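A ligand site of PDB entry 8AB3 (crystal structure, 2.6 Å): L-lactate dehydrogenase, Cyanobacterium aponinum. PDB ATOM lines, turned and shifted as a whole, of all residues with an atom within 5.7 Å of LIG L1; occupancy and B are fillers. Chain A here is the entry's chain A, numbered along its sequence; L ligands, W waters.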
ATOM      1  N   ILE A  26      -0.087 -19.113  18.155  1.00  0.00           N
ATOM      2  CA  ILE A  26      -0.386 -20.521  18.403  1.00  0.00           C
ATOM      3  C   ILE A  26      -0.870 -20.674  19.836  1.00  0.00           C
ATOM      4  O   ILE A  26      -0.106 -20.416  20.770  1.00  0.00           O
ATOM      5  CB  ILE A  26       0.843 -21.417  18.149  1.00  0.00           C
ATOM      6  CG1 ILE A  26       1.421 -21.149  16.729  1.00  0.00           C
ATOM      7  CG2 ILE A  26       0.490 -22.897  18.376  1.00  0.00           C
ATOM      8  CD1 ILE A  26       2.697 -21.860  16.459  1.00  0.00           C
ATOM      9  N   GLY A  27      -2.126 -21.062  19.977  1.00  0.00           N
ATOM     10  CA  GLY A  27      -2.807 -21.183  21.264  1.00  0.00           C
ATOM     11  C   GLY A  27      -3.686 -19.970  21.496  1.00  0.00           C
ATOM     12  O   GLY A  27      -3.179 -18.863  21.746  1.00  0.00           O
ATOM     13  N   LEU A  28      -5.003 -20.138  21.357  1.00  0.00           N
ATOM     14  CA  LEU A  28      -5.913 -19.031  21.531  1.00  0.00           C
ATOM     15  C   LEU A  28      -6.910 -19.183  22.662  1.00  0.00           C
ATOM     16  O   LEU A  28      -8.110 -19.130  22.462  1.00  0.00           O
ATOM     17  CB  LEU A  28      -6.607 -18.674  20.219  1.00  0.00           C
ATOM     18  CG  LEU A  28      -5.690 -17.807  19.403  1.00  0.00           C
ATOM     19  CD1 LEU A  28      -5.166 -18.552  18.213  1.00  0.00           C
ATOM     20  CD2 LEU A  28      -6.302 -16.452  19.118  1.00  0.00           C
ATOM     21  N   GLY A  29      -6.379 -19.244  23.876  1.00  0.00           N
ATOM     22  CA  GLY A  29      -7.205 -19.235  25.073  1.00  0.00           C
ATOM     23  C   GLY A  29      -7.306 -17.820  25.562  1.00  0.00           C
ATOM     24  O   GLY A  29      -7.309 -16.875  24.763  1.00  0.00           O
ATOM     25  N   GLN A  30      -7.354 -17.630  26.873  1.00  0.00           N
ATOM     26  CA  GLN A  30      -7.466 -16.290  27.468  1.00  0.00           C
ATOM     27  C   GLN A  30      -6.346 -15.350  27.081  1.00  0.00           C
ATOM     28  O   GLN A  30      -6.610 -14.195  26.781  1.00  0.00           O
ATOM     29  CB  GLN A  30      -7.600 -16.371  28.986  1.00  0.00           C
ATOM     30  CG  GLN A  30      -8.778 -17.210  29.452  1.00  0.00           C
ATOM     31  CD  GLN A  30     -10.130 -16.603  29.169  1.00  0.00           C
ATOM     32  OE1 GLN A  30     -10.283 -15.411  28.869  1.00  0.00           O
ATOM     33  NE2 GLN A  30     -11.157 -17.422  29.266  1.00  0.00           N
ATOM     34  N   VAL A  31      -5.104 -15.827  27.093  1.00  0.00           N
ATOM     35  CA  VAL A  31      -3.943 -15.008  26.772  1.00  0.00           C
ATOM     36  C   VAL A  31      -3.866 -14.721  25.266  1.00  0.00           C
ATOM     37  O   VAL A  31      -3.765 -13.568  24.860  1.00  0.00           O
ATOM     38  CB  VAL A  31      -2.638 -15.666  27.307  1.00  0.00           C
ATOM     39  CG1 VAL A  31      -1.393 -14.934  26.811  1.00  0.00           C
ATOM     40  CG2 VAL A  31      -2.656 -15.781  28.834  1.00  0.00           C
ATOM     41  N   GLY A  32      -3.956 -15.776  24.447  1.00  0.00           N
ATOM     42  CA  GLY A  32      -3.947 -15.693  22.995  1.00  0.00           C
ATOM     43  C   GLY A  32      -5.047 -14.813  22.431  1.00  0.00           C
ATOM     44  O   GLY A  32      -4.813 -14.114  21.456  1.00  0.00           O
ATOM     45  N   GLN A  51      -3.849 -20.176  15.324  1.00  0.00           N
ATOM     46  CA  GLN A  51      -3.771 -21.638  15.341  1.00  0.00           C
ATOM     47  C   GLN A  51      -4.144 -22.210  16.702  1.00  0.00           C
ATOM     48  O   GLN A  51      -3.525 -21.852  17.707  1.00  0.00           O
ATOM     49  CB  GLN A  51      -2.364 -22.109  14.934  1.00  0.00           C
ATOM     50  CG  GLN A  51      -2.128 -23.620  15.053  1.00  0.00           C
ATOM     51  CD  GLN A  51      -0.734 -24.029  14.565  1.00  0.00           C
ATOM     52  OE1 GLN A  51      -0.233 -23.551  13.556  1.00  0.00           O
ATOM     53  NE2 GLN A  51      -0.090 -24.925  15.291  1.00  0.00           N
ATOM     54  N   ASP A  52      -5.128 -23.132  16.747  1.00  0.00           N
ATOM     55  CA  ASP A  52      -5.534 -23.787  17.990  1.00  0.00           C
ATOM     56  C   ASP A  52      -6.128 -25.172  17.714  1.00  0.00           C
ATOM     57  O   ASP A  52      -6.759 -25.374  16.673  1.00  0.00           O
ATOM     58  CB  ASP A  52      -6.570 -22.938  18.769  1.00  0.00           C
ATOM     59  CG  ASP A  52      -6.633 -23.261  20.250  1.00  0.00           C
ATOM     60  OD1 ASP A  52      -7.078 -24.363  20.588  1.00  0.00           O
ATOM     61  OD2 ASP A  52      -6.239 -22.422  21.043  1.00  0.00           O
ATOM     62  N   ILE A  53      -5.970 -26.096  18.661  1.00  0.00           N
ATOM     63  CA  ILE A  53      -6.539 -27.440  18.567  1.00  0.00           C
ATOM     64  C   ILE A  53      -8.063 -27.467  18.799  1.00  0.00           C
ATOM     65  O   ILE A  53      -8.715 -28.440  18.428  1.00  0.00           O
ATOM     66  CB  ILE A  53      -5.779 -28.420  19.488  1.00  0.00           C
ATOM     67  CG1 ILE A  53      -5.740 -27.888  20.936  1.00  0.00           C
ATOM     68  CG2 ILE A  53      -4.380 -28.674  18.950  1.00  0.00           C
ATOM     69  CD1 ILE A  53      -5.211 -28.863  21.928  1.00  0.00           C
ATOM     70  N   ALA A  54      -8.628 -26.419  19.414  1.00  0.00           N
ATOM     71  CA  ALA A  54     -10.080 -26.310  19.641  1.00  0.00           C
ATOM     72  C   ALA A  54     -10.685 -25.591  18.443  1.00  0.00           C
ATOM     73  O   ALA A  54     -10.873 -24.378  18.466  1.00  0.00           O
ATOM     74  CB  ALA A  54     -10.365 -25.529  20.915  1.00  0.00           C
ATOM     75  N   THR A  95       1.473 -19.084  22.856  1.00  0.00           N
ATOM     76  CA  THR A  95       0.854 -19.001  24.175  1.00  0.00           C
ATOM     77  C   THR A  95       0.296 -20.378  24.607  1.00  0.00           C
ATOM     78  O   THR A  95       0.009 -20.551  25.783  1.00  0.00           O
ATOM     79  CB  THR A  95      -0.274 -17.948  24.229  1.00  0.00           C
ATOM     80  OG1 THR A  95      -1.506 -18.538  23.782  1.00  0.00           O
ATOM     81  CG2 THR A  95       0.047 -16.673  23.491  1.00  0.00           C
ATOM     82  N   ALA A  96       0.102 -21.340  23.648  1.00  0.00           N
ATOM     83  CA  ALA A  96      -0.444 -22.674  23.874  1.00  0.00           C
ATOM     84  C   ALA A  96       0.140 -23.353  25.102  1.00  0.00           C
ATOM     85  O   ALA A  96       1.354 -23.295  25.303  1.00  0.00           O
ATOM     86  CB  ALA A  96      -0.210 -23.542  22.650  1.00  0.00           C
ATOM     87  N   GLY A  97      -0.711 -23.975  25.905  1.00  0.00           N
ATOM     88  CA  GLY A  97      -0.258 -24.678  27.104  1.00  0.00           C
ATOM     89  C   GLY A  97      -1.200 -24.633  28.291  1.00  0.00           C
ATOM     90  O   GLY A  97      -2.261 -24.020  28.222  1.00  0.00           O
ATOM     91  N   VAL A  98      -0.830 -25.314  29.387  1.00  0.00           N
ATOM     92  CA  VAL A  98      -1.667 -25.331  30.576  1.00  0.00           C
ATOM     93  C   VAL A  98      -1.380 -24.124  31.443  1.00  0.00           C
ATOM     94  O   VAL A  98      -0.217 -23.728  31.612  1.00  0.00           O
ATOM     95  CB  VAL A  98      -1.627 -26.661  31.369  1.00  0.00           C
ATOM     96  CG1 VAL A  98      -2.041 -27.823  30.483  1.00  0.00           C
ATOM     97  CG2 VAL A  98      -0.262 -26.908  31.996  1.00  0.00           C
ATOM     98  N   ALA A  99      -2.442 -23.498  31.961  1.00  0.00           N
ATOM     99  CA  ALA A  99      -2.301 -22.371  32.873  1.00  0.00           C
ATOM    100  C   ALA A  99      -2.303 -22.879  34.319  1.00  0.00           C
ATOM    101  O   ALA A  99      -2.827 -23.978  34.585  1.00  0.00           O
ATOM    102  CB  ALA A  99      -3.399 -21.344  32.650  1.00  0.00           C
ATOM    103  N   GLN A 100      -1.730 -22.111  35.232  1.00  0.00           N
ATOM    104  CA  GLN A 100      -1.647 -22.543  36.630  1.00  0.00           C
ATOM    105  C   GLN A 100      -2.988 -22.383  37.373  1.00  0.00           C
ATOM    106  O   GLN A 100      -3.736 -21.432  37.167  1.00  0.00           O
ATOM    107  CB  GLN A 100      -0.461 -21.872  37.373  1.00  0.00           C
ATOM    108  CG  GLN A 100      -0.754 -20.553  38.063  1.00  0.00           C
ATOM    109  CD  GLN A 100       0.423 -19.594  38.044  1.00  0.00           C
ATOM    110  OE1 GLN A 100       0.366 -18.494  37.478  1.00  0.00           O
ATOM    111  NE2 GLN A 100       1.510 -19.962  38.682  1.00  0.00           N
ATOM    112  N   ARG A 106       4.286 -21.819  38.652  1.00  0.00           N
ATOM    113  CA  ARG A 106       4.488 -21.844  37.200  1.00  0.00           C
ATOM    114  C   ARG A 106       5.418 -23.014  36.854  1.00  0.00           C
ATOM    115  O   ARG A 106       5.185 -23.701  35.851  1.00  0.00           O
ATOM    116  CB  ARG A 106       5.113 -20.524  36.720  1.00  0.00           C
ATOM    117  CG  ARG A 106       4.126 -19.368  36.668  1.00  0.00           C
ATOM    118  CD  ARG A 106       4.872 -18.107  36.312  1.00  0.00           C
ATOM    119  NE  ARG A 106       4.181 -16.853  36.628  1.00  0.00           N
ATOM    120  CZ  ARG A 106       4.141 -16.297  37.832  1.00  0.00           C
ATOM    121  NH1 ARG A 106       3.557 -15.120  38.002  1.00  0.00           N
ATOM    122  NH2 ARG A 106       4.668 -16.916  38.880  1.00  0.00           N
ATOM    123  N   LEU A 109       4.160 -26.529  35.758  1.00  0.00           N
ATOM    124  CA  LEU A 109       3.512 -26.717  34.452  1.00  0.00           C
ATOM    125  C   LEU A 109       4.512 -27.217  33.390  1.00  0.00           C
ATOM    126  O   LEU A 109       4.074 -27.583  32.303  1.00  0.00           O
ATOM    127  CB  LEU A 109       2.909 -25.397  33.939  1.00  0.00           C
ATOM    128  CG  LEU A 109       2.101 -24.580  34.920  1.00  0.00           C
ATOM    129  CD1 LEU A 109       2.027 -23.122  34.478  1.00  0.00           C
ATOM    130  CD2 LEU A 109       0.726 -25.155  35.097  1.00  0.00           C
ATOM    131  N   ASN A 113       3.927 -28.698  29.498  1.00  0.00           N
ATOM    132  CA  ASN A 113       4.092 -27.742  28.400  1.00  0.00           C
ATOM    133  C   ASN A 113       5.234 -28.100  27.450  1.00  0.00           C
ATOM    134  O   ASN A 113       5.100 -27.800  26.257  1.00  0.00           O
ATOM    135  CB  ASN A 113       4.189 -26.317  28.934  1.00  0.00           C
ATOM    136  CG  ASN A 113       2.845 -25.844  29.450  1.00  0.00           C
ATOM    137  OD1 ASN A 113       1.787 -26.326  29.046  1.00  0.00           O
ATOM    138  ND2 ASN A 113       2.824 -24.899  30.365  1.00  0.00           N
ATOM    139  N   ILE A 116       3.661 -30.342  24.859  1.00  0.00           N
ATOM    140  CA  ILE A 116       2.859 -29.590  23.899  1.00  0.00           C
ATOM    141  C   ILE A 116       3.768 -28.936  22.843  1.00  0.00           C
ATOM    142  O   ILE A 116       3.419 -28.915  21.666  1.00  0.00           O
ATOM    143  CB  ILE A 116       1.981 -28.542  24.645  1.00  0.00           C
ATOM    144  CG1 ILE A 116       0.871 -29.227  25.460  1.00  0.00           C
ATOM    145  CG2 ILE A 116       1.408 -27.464  23.706  1.00  0.00           C
ATOM    146  CD1 ILE A 116       0.072 -28.294  26.375  1.00  0.00           C
ATOM    147  N   LYS A 119       5.214 -31.114  19.824  1.00  0.00           N
ATOM    148  CA  LYS A 119       4.306 -31.273  18.701  1.00  0.00           C
ATOM    149  C   LYS A 119       4.359 -30.037  17.784  1.00  0.00           C
ATOM    150  O   LYS A 119       4.437 -30.185  16.567  1.00  0.00           O
ATOM    151  CB  LYS A 119       2.874 -31.458  19.230  1.00  0.00           C
ATOM    152  CG  LYS A 119       2.746 -32.557  20.269  1.00  0.00           C
ATOM    153  CD  LYS A 119       1.449 -32.452  21.064  1.00  0.00           C
ATOM    154  CE  LYS A 119       1.429 -33.503  22.157  1.00  0.00           C
ATOM    155  NZ  LYS A 119       0.091 -33.621  22.812  1.00  0.00           N
ATOM    156  N   ILE A 120       4.376 -28.835  18.376  1.00  0.00           N
ATOM    157  CA  ILE A 120       4.375 -27.551  17.664  1.00  0.00           C
ATOM    158  C   ILE A 120       5.689 -27.145  16.973  1.00  0.00           C
ATOM    159  O   ILE A 120       5.644 -26.792  15.793  1.00  0.00           O
ATOM    160  CB  ILE A 120       3.915 -26.418  18.622  1.00  0.00           C
ATOM    161  CG1 ILE A 120       2.573 -26.723  19.299  1.00  0.00           C
ATOM    162  CG2 ILE A 120       3.898 -25.065  17.911  1.00  0.00           C
ATOM    163  CD1 ILE A 120       2.287 -25.736  20.466  1.00  0.00           C
ATOM    164  N   VAL A 135       7.860 -16.549  22.984  1.00  0.00           N
ATOM    165  CA  VAL A 135       7.316 -17.533  23.937  1.00  0.00           C
ATOM    166  C   VAL A 135       6.610 -16.885  25.128  1.00  0.00           C
ATOM    167  O   VAL A 135       7.199 -16.052  25.813  1.00  0.00           O
ATOM    168  CB  VAL A 135       8.461 -18.470  24.388  1.00  0.00           C
ATOM    169  CG1 VAL A 135       7.957 -19.536  25.352  1.00  0.00           C
ATOM    170  CG2 VAL A 135       9.144 -19.125  23.191  1.00  0.00           C
ATOM    171  N   VAL A 136       5.350 -17.264  25.393  1.00  0.00           N
ATOM    172  CA  VAL A 136       4.564 -16.724  26.515  1.00  0.00           C
ATOM    173  C   VAL A 136       4.219 -17.814  27.545  1.00  0.00           C
ATOM    174  O   VAL A 136       4.109 -17.523  28.734  1.00  0.00           O
ATOM    175  CB  VAL A 136       3.305 -15.976  25.989  1.00  0.00           C
ATOM    176  CG1 VAL A 136       2.480 -15.379  27.137  1.00  0.00           C
ATOM    177  CG2 VAL A 136       3.687 -14.893  24.985  1.00  0.00           C
ATOM    178  N   THR A 137       4.055 -19.075  27.087  1.00  0.00           N
ATOM    179  CA  THR A 137       3.742 -20.242  27.913  1.00  0.00           C
ATOM    180  C   THR A 137       4.655 -20.348  29.133  1.00  0.00           C
ATOM    181  O   THR A 137       5.849 -20.060  29.015  1.00  0.00           O
ATOM    182  CB  THR A 137       3.893 -21.526  27.071  1.00  0.00           C
ATOM    183  OG1 THR A 137       3.179 -21.400  25.838  1.00  0.00           O
ATOM    184  CG2 THR A 137       3.440 -22.743  27.790  1.00  0.00           C
ATOM    185  N   ASN A 138       4.093 -20.742  30.287  1.00  0.00           N
ATOM    186  CA  ASN A 138       4.818 -20.854  31.546  1.00  0.00           C
ATOM    187  C   ASN A 138       5.381 -22.262  31.839  1.00  0.00           C
ATOM    188  O   ASN A 138       4.766 -23.232  31.436  1.00  0.00           O
ATOM    189  CB  ASN A 138       3.885 -20.423  32.673  1.00  0.00           C
ATOM    190  CG  ASN A 138       3.953 -18.975  33.004  1.00  0.00           C
ATOM    191  OD1 ASN A 138       4.999 -18.339  32.892  1.00  0.00           O
ATOM    192  ND2 ASN A 138       2.841 -18.417  33.453  1.00  0.00           N
ATOM    193  N   VAL A 140       7.802 -19.422  31.665  1.00  0.00           N
ATOM    194  CA  VAL A 140       8.267 -18.640  30.527  1.00  0.00           C
ATOM    195  C   VAL A 140       9.773 -18.741  30.265  1.00  0.00           C
ATOM    196  O   VAL A 140      10.158 -18.849  29.100  1.00  0.00           O
ATOM    197  CB  VAL A 140       7.791 -17.148  30.567  1.00  0.00           C
ATOM    198  CG1 VAL A 140       8.807 -16.213  31.217  1.00  0.00           C
ATOM    199  CG2 VAL A 140       7.439 -16.656  29.171  1.00  0.00           C
ATOM    200  N   SER A 161       8.543 -13.596  26.817  1.00  0.00           N
ATOM    201  CA  SER A 161       7.928 -12.366  27.323  1.00  0.00           C
ATOM    202  C   SER A 161       8.555 -11.903  28.665  1.00  0.00           C
ATOM    203  O   SER A 161       8.596 -10.715  28.954  1.00  0.00           O
ATOM    204  CB  SER A 161       6.407 -12.503  27.415  1.00  0.00           C
ATOM    205  OG  SER A 161       6.042 -13.463  28.384  1.00  0.00           O
ATOM    206  N   GLY A 162       9.069 -12.854  29.427  1.00  0.00           N
ATOM    207  CA  GLY A 162       9.796 -12.616  30.661  1.00  0.00           C
ATOM    208  C   GLY A 162       9.207 -11.684  31.683  1.00  0.00           C
ATOM    209  O   GLY A 162       8.068 -11.856  32.107  1.00  0.00           O
ATOM    210  N   LEU A 165       6.016  -7.889  31.898  1.00  0.00           N
ATOM    211  CA  LEU A 165       4.781  -7.847  32.692  1.00  0.00           C
ATOM    212  C   LEU A 165       5.053  -7.497  34.163  1.00  0.00           C
ATOM    213  O   LEU A 165       4.390  -6.616  34.707  1.00  0.00           O
ATOM    214  CB  LEU A 165       4.064  -9.211  32.583  1.00  0.00           C
ATOM    215  CG  LEU A 165       2.745  -9.351  33.326  1.00  0.00           C
ATOM    216  CD1 LEU A 165       1.784  -8.240  32.967  1.00  0.00           C
ATOM    217  CD2 LEU A 165       2.128 -10.686  33.038  1.00  0.00           C
ATOM    218  N   HIS A 193      10.384 -14.998  35.734  1.00  0.00           N
ATOM    219  CA  HIS A 193       9.019 -14.503  35.794  1.00  0.00           C
ATOM    220  C   HIS A 193       8.358 -15.494  36.768  1.00  0.00           C
ATOM    221  O   HIS A 193       7.835 -16.525  36.363  1.00  0.00           O
ATOM    222  CB  HIS A 193       8.335 -14.568  34.430  1.00  0.00           C
ATOM    223  CG  HIS A 193       6.864 -14.290  34.470  1.00  0.00           C
ATOM    224  ND1 HIS A 193       6.374 -13.032  34.749  1.00  0.00           N
ATOM    225  CD2 HIS A 193       5.817 -15.118  34.232  1.00  0.00           C
ATOM    226  CE1 HIS A 193       5.060 -13.140  34.681  1.00  0.00           C
ATOM    227  NE2 HIS A 193       4.688 -14.372  34.375  1.00  0.00           N
ATOM    228  N   TYR A 247      -7.721 -16.509  36.107  1.00  0.00           N
ATOM    229  CA  TYR A 247      -6.606 -16.434  35.165  1.00  0.00           C
ATOM    230  C   TYR A 247      -6.184 -14.956  34.990  1.00  0.00           C
ATOM    231  O   TYR A 247      -6.815 -14.069  35.559  1.00  0.00           O
ATOM    232  CB  TYR A 247      -7.062 -17.008  33.788  1.00  0.00           C
ATOM    233  CG  TYR A 247      -8.241 -16.245  33.215  1.00  0.00           C
ATOM    234  CD1 TYR A 247      -9.546 -16.595  33.533  1.00  0.00           C
ATOM    235  CD2 TYR A 247      -8.044 -15.130  32.398  1.00  0.00           C
ATOM    236  CE1 TYR A 247     -10.623 -15.854  33.073  1.00  0.00           C
ATOM    237  CE2 TYR A 247      -9.117 -14.390  31.921  1.00  0.00           C
ATOM    238  CZ  TYR A 247     -10.407 -14.763  32.250  1.00  0.00           C
ATOM    239  OH  TYR A 247     -11.467 -14.026  31.776  1.00  0.00           O
ATOM    240  N   THR A 248      -5.132 -14.693  34.195  1.00  0.00           N
ATOM    241  CA  THR A 248      -4.719 -13.326  33.837  1.00  0.00           C
ATOM    242  C   THR A 248      -4.632 -13.265  32.285  1.00  0.00           C
ATOM    243  O   THR A 248      -4.221 -14.254  31.656  1.00  0.00           O
ATOM    244  CB  THR A 248      -3.432 -12.862  34.572  1.00  0.00           C
ATOM    245  OG1 THR A 248      -2.261 -13.184  33.818  1.00  0.00           O
ATOM    246  CG2 THR A 248      -3.323 -13.379  36.008  1.00  0.00           C
ATOM    247  N   SER A 249      -5.006 -12.119  31.657  1.00  0.00           N
ATOM    248  CA  SER A 249      -4.970 -12.029  30.194  1.00  0.00           C
ATOM    249  C   SER A 249      -4.678 -10.626  29.624  1.00  0.00           C
ATOM    250  O   SER A 249      -3.901 -10.507  28.680  1.00  0.00           O
ATOM    251  CB  SER A 249      -6.266 -12.557  29.600  1.00  0.00           C
ATOM    252  OG  SER A 249      -7.394 -11.804  30.029  1.00  0.00           O
ATOM    253  N   ILE A 252      -0.881  -9.142  30.041  1.00  0.00           N
ATOM    254  CA  ILE A 252       0.057  -9.929  29.226  1.00  0.00           C
ATOM    255  C   ILE A 252      -0.186  -9.701  27.743  1.00  0.00           C
ATOM    256  O   ILE A 252       0.768  -9.678  26.972  1.00  0.00           O
ATOM    257  CB  ILE A 252       0.135 -11.445  29.605  1.00  0.00           C
ATOM    258  CG1 ILE A 252       1.261 -12.173  28.826  1.00  0.00           C
ATOM    259  CG2 ILE A 252      -1.181 -12.169  29.432  1.00  0.00           C
ATOM    260  CD1 ILE A 252       2.665 -11.646  29.053  1.00  0.00           C
HETATM  261  P1  LIG L   1      -5.962 -21.533  28.280  1.00  0.00           P
HETATM  262  O1  LIG L   1      -6.230 -22.909  28.736  1.00  0.00           O
HETATM  263  O2  LIG L   1      -7.234 -20.733  28.004  1.00  0.00           O
HETATM  264  O3  LIG L   1      -5.059 -21.467  26.975  1.00  0.00           O
HETATM  265  C1  LIG L   1      -4.317 -22.546  26.370  1.00  0.00           C
HETATM  266  C2  LIG L   1      -4.754 -22.648  24.933  1.00  0.00           C
HETATM  267  O4  LIG L   1      -3.771 -23.399  24.175  1.00  0.00           O
HETATM  268  C3  LIG L   1      -6.112 -23.325  24.696  1.00  0.00           C
HETATM  269  O5  LIG L   1      -6.858 -22.543  23.772  1.00  0.00           O
HETATM  270  C4  LIG L   1      -5.712 -24.675  24.091  1.00  0.00           C
HETATM  271  O6  LIG L   1      -6.684 -25.251  23.211  1.00  0.00           O
HETATM  272  C5  LIG L   1      -4.475 -24.273  23.317  1.00  0.00           C
HETATM  273  N1  LIG L   1      -3.600 -25.373  22.951  1.00  0.00           N
HETATM  274  C6  LIG L   1      -3.151 -26.404  23.730  1.00  0.00           C
HETATM  275  N2  LIG L   1      -2.356 -27.234  23.108  1.00  0.00           N
HETATM  276  C7  LIG L   1      -2.274 -26.728  21.830  1.00  0.00           C
HETATM  277  C8  LIG L   1      -1.529 -27.110  20.694  1.00  0.00           C
HETATM  278  N3  LIG L   1      -0.771 -28.203  20.645  1.00  0.00           N
HETATM  279  N4  LIG L   1      -1.588 -26.310  19.601  1.00  0.00           N
HETATM  280  C9  LIG L   1      -2.374 -25.228  19.638  1.00  0.00           C
HETATM  281  N5  LIG L   1      -3.140 -24.786  20.631  1.00  0.00           N
HETATM  282  C10 LIG L   1      -3.038 -25.572  21.710  1.00  0.00           C
HETATM  283  O7  LIG L   1      -5.111 -20.738  29.357  1.00  0.00           O
HETATM  284  P2  LIG L   1      -4.278 -19.380  29.316  1.00  0.00           P
HETATM  285  O8  LIG L   1      -4.718 -18.535  30.546  1.00  0.00           O
HETATM  286  O9  LIG L   1      -4.390 -18.711  27.988  1.00  0.00           O
HETATM  287  O10 LIG L   1      -2.727 -19.736  29.497  1.00  0.00           O
HETATM  288  C11 LIG L   1      -1.818 -20.013  28.414  1.00  0.00           C
HETATM  289  C12 LIG L   1      -0.405 -20.126  28.949  1.00  0.00           C
HETATM  290  O11 LIG L   1       0.150 -18.802  29.117  1.00  0.00           O
HETATM  291  C13 LIG L   1      -0.238 -20.827  30.295  1.00  0.00           C
HETATM  292  O12 LIG L   1       0.927 -21.646  30.286  1.00  0.00           O
HETATM  293  C14 LIG L   1      -0.082 -19.659  31.276  1.00  0.00           C
HETATM  294  O13 LIG L   1       0.600 -19.986  32.477  1.00  0.00           O
HETATM  295  C15 LIG L   1       0.730 -18.712  30.409  1.00  0.00           C
HETATM  296  N6  LIG L   1       0.743 -17.318  30.836  1.00  0.00           N
HETATM  297  C16 LIG L   1       1.944 -16.605  30.823  1.00  0.00           C
HETATM  298  C17 LIG L   1       2.041 -15.322  31.206  1.00  0.00           C
HETATM  299  C18 LIG L   1       3.376 -14.689  31.219  1.00  0.00           C
HETATM  300  O14 LIG L   1       3.600 -13.725  31.959  1.00  0.00           O
HETATM  301  N7  LIG L   1       4.310 -15.206  30.427  1.00  0.00           N
HETATM  302  C19 LIG L   1       0.823 -14.544  31.661  1.00  0.00           C
HETATM  303  C20 LIG L   1      -0.408 -15.404  31.647  1.00  0.00           C
HETATM  304  C21 LIG L   1      -0.398 -16.683  31.252  1.00  0.00           C
HETATM  305  C1  LG2 L   2       1.096 -15.411  35.038  1.00  0.00           C
HETATM  306  N1  LG2 L   2      -0.125 -15.882  34.769  1.00  0.00           N
HETATM  307  O1  LG2 L   2       2.114 -16.082  34.891  1.00  0.00           O
HETATM  308  C2  LG2 L   2       1.182 -13.927  35.450  1.00  0.00           C
HETATM  309  O2  LG2 L   2       0.068 -13.236  35.355  1.00  0.00           O
HETATM  310  O3  LG2 L   2       2.215 -13.454  35.919  1.00  0.00           O
HETATM  311  O   HOH W   1       5.749 -12.325  30.720  1.00  0.00           O
HETATM  312  O   HOH W   2      -3.932 -18.499  25.363  1.00  0.00           O
HETATM  313  O   HOH W   3      -5.239 -24.083  31.219  1.00  0.00           O
HETATM  314  O   HOH W   4      -1.495 -27.090  16.654  1.00  0.00           O
HETATM  315  O   HOH W   5      -8.307 -27.207  24.543  1.00  0.00           O
HETATM  316  O   HOH W   6      -3.458 -17.345  32.644  1.00  0.00           O
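The backbone NH (N) of Asn 138 lies within hydrogen-bond range of an oxygen (O12) of LIG L1, 3.3 Å away. O of Val 136 sits at hydrogen-bond distance from N7 of LIG L1, at 2.9 Å. The side-chain amide nitrogen of Asn 138 sits at hydrogen-bond distance from an oxygen (O1) of LG2 L2, 2.8 Å away. An oxygen (O6) of LIG L1 lies within hydrogen-bond range of the side-chain carboxylate (OD1) of Asp 52 (2.8 Å). The side-chain hydroxyl (OG1) of Thr 248 lies within hydrogen-bond range of an oxygen (O2) of LG2 L2 (2.8 Å). A ring nitrogen (NE2) of His 193 is in hydrogen-bond range of an oxygen (O14) of LIG L1. The backbone NH (N) of Gln 30 lies within hydrogen-bond range of an oxygen (O2) of LIG L1, at 3.3 Å. OG of Ser 161 sits at hydrogen-bond distance from N7 of LIG L1. The backbone NH of Gly 29 lies within hydrogen-bond range of an oxygen (O5) of LIG L1. An oxygen (O13) of LIG L1 lies within hydrogen-bond range of the side-chain amide nitrogen of Asn 138, at 2.9 Å. A ring nitrogen (NE2) of His 193 is in hydrogen-bond range of an oxygen (O3) of LG2 L2 (3.1 Å). O12 of LIG L1 lies within hydrogen-bond range of O of Val 98 (2.7 Å). The backbone NH (N) of Val 31 lies within hydrogen-bond range of an oxygen (O9) of LIG L1. NH1 of Arg 106 lies within salt-bridge range of O3 of LG2 L2 (3.0 Å).
The side-chain amide oxygen (OD1) of Asn 113 is in hydrogen-bond range of the backbone NH (N) of Val 98 (2.8 Å). The backbone NH of Gly 27 is in hydrogen-bond range of the backbone carbonyl oxygen of Gln 51 (2.8 Å). OD1 of Asp 52 sits at hydrogen-bond distance from N of Ala 54. A ring nitrogen (ND1) of His 193 is in hydrogen-bond range of the backbone carbonyl oxygen of Gly 162 (3.4 Å). OG1 of Thr 95 is in hydrogen-bond range of O of Gly 27. The guanidinium group of Arg 106 sits close to a ring nitrogen (NE2) of His 193 (3.4 Å). The backbone carbonyl oxygen (O) of Asn 138 sits at hydrogen-bond distance from the side-chain amide nitrogen (ND2) of Asn 113, at 2.8 Å. The backbone NH (N) of Ser 161 sits at hydrogen-bond distance from the backbone carbonyl oxygen (O) of Val 135 (3.0 Å).
Water W6 bridges O8 of LIG L1 (2.7 Å) and O of Thr 248 (3.3 Å). Water W1 lies within hydrogen-bond range of OG of Ser 161 (2.6 Å), O of Gly 162 (2.7 Å) and O14 of LIG L1 (2.8 Å). Water W3 bridges O1 of LIG L1 and N of Ala 99. Water W4 lies within hydrogen-bond range of the side-chain amide nitrogen of Gln 51 and a nitrogen (N4) of LIG L1.
CG2 of Ile 26 touches C9 of LIG L1, 3.9 Å away. Gly 27 touches LIG L1 (CA to N5, 3.7 Å). C of Leu 28 touches O5 of LIG L1 (3.5 Å). CD1 of Ile 53 touches N2 of LIG L1, at 3.5 Å. Thr 95 touches LIG L1 (O to C12, 3.2 Å). CA of Ala 96 touches O4 of LIG L1, at 3.4 Å. Gly 97 touches LIG L1. CB of Ala 99 touches O10 of LIG L1 (3.6 Å). Leu 109 touches LIG L1. ND2 of Asn 113 touches O12 of LIG L1, 3.8 Å away. CG2 of Ile 116 touches N2 of LIG L1, 3.8 Å away. Ile 120 touches LIG L1. CG2 of Thr 137 touches O12 of LIG L1 (3.7 Å). CG2 of Val 140 touches N7 of LIG L1, at 3.7 Å. Leu 165 touches LIG L1 (CD2 to O14, 3.5 Å). Thr 248 touches LIG L1 (OG1 to C20, 3.6 Å). CD1 of Ile 252 touches O14 of LIG L1 (3.7 Å). Hydrophobic or aromatic side chains that line LIG L1: Ile 26, Val 31, Ile 53, Ala 96, Ala 99, Leu 109, Ile 116, Ile 120, Val 136, Val 140, Leu 165, His 193 and Ile 252. Of the 36 residues printed, 26 come within 4 Å of LIG L1. Along chain A the residues within 4 Å of LIG L1 span positions 26 to 252. The nearest printed residue that does not touch LIG L1 is Gln 51 (4.1 Å).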
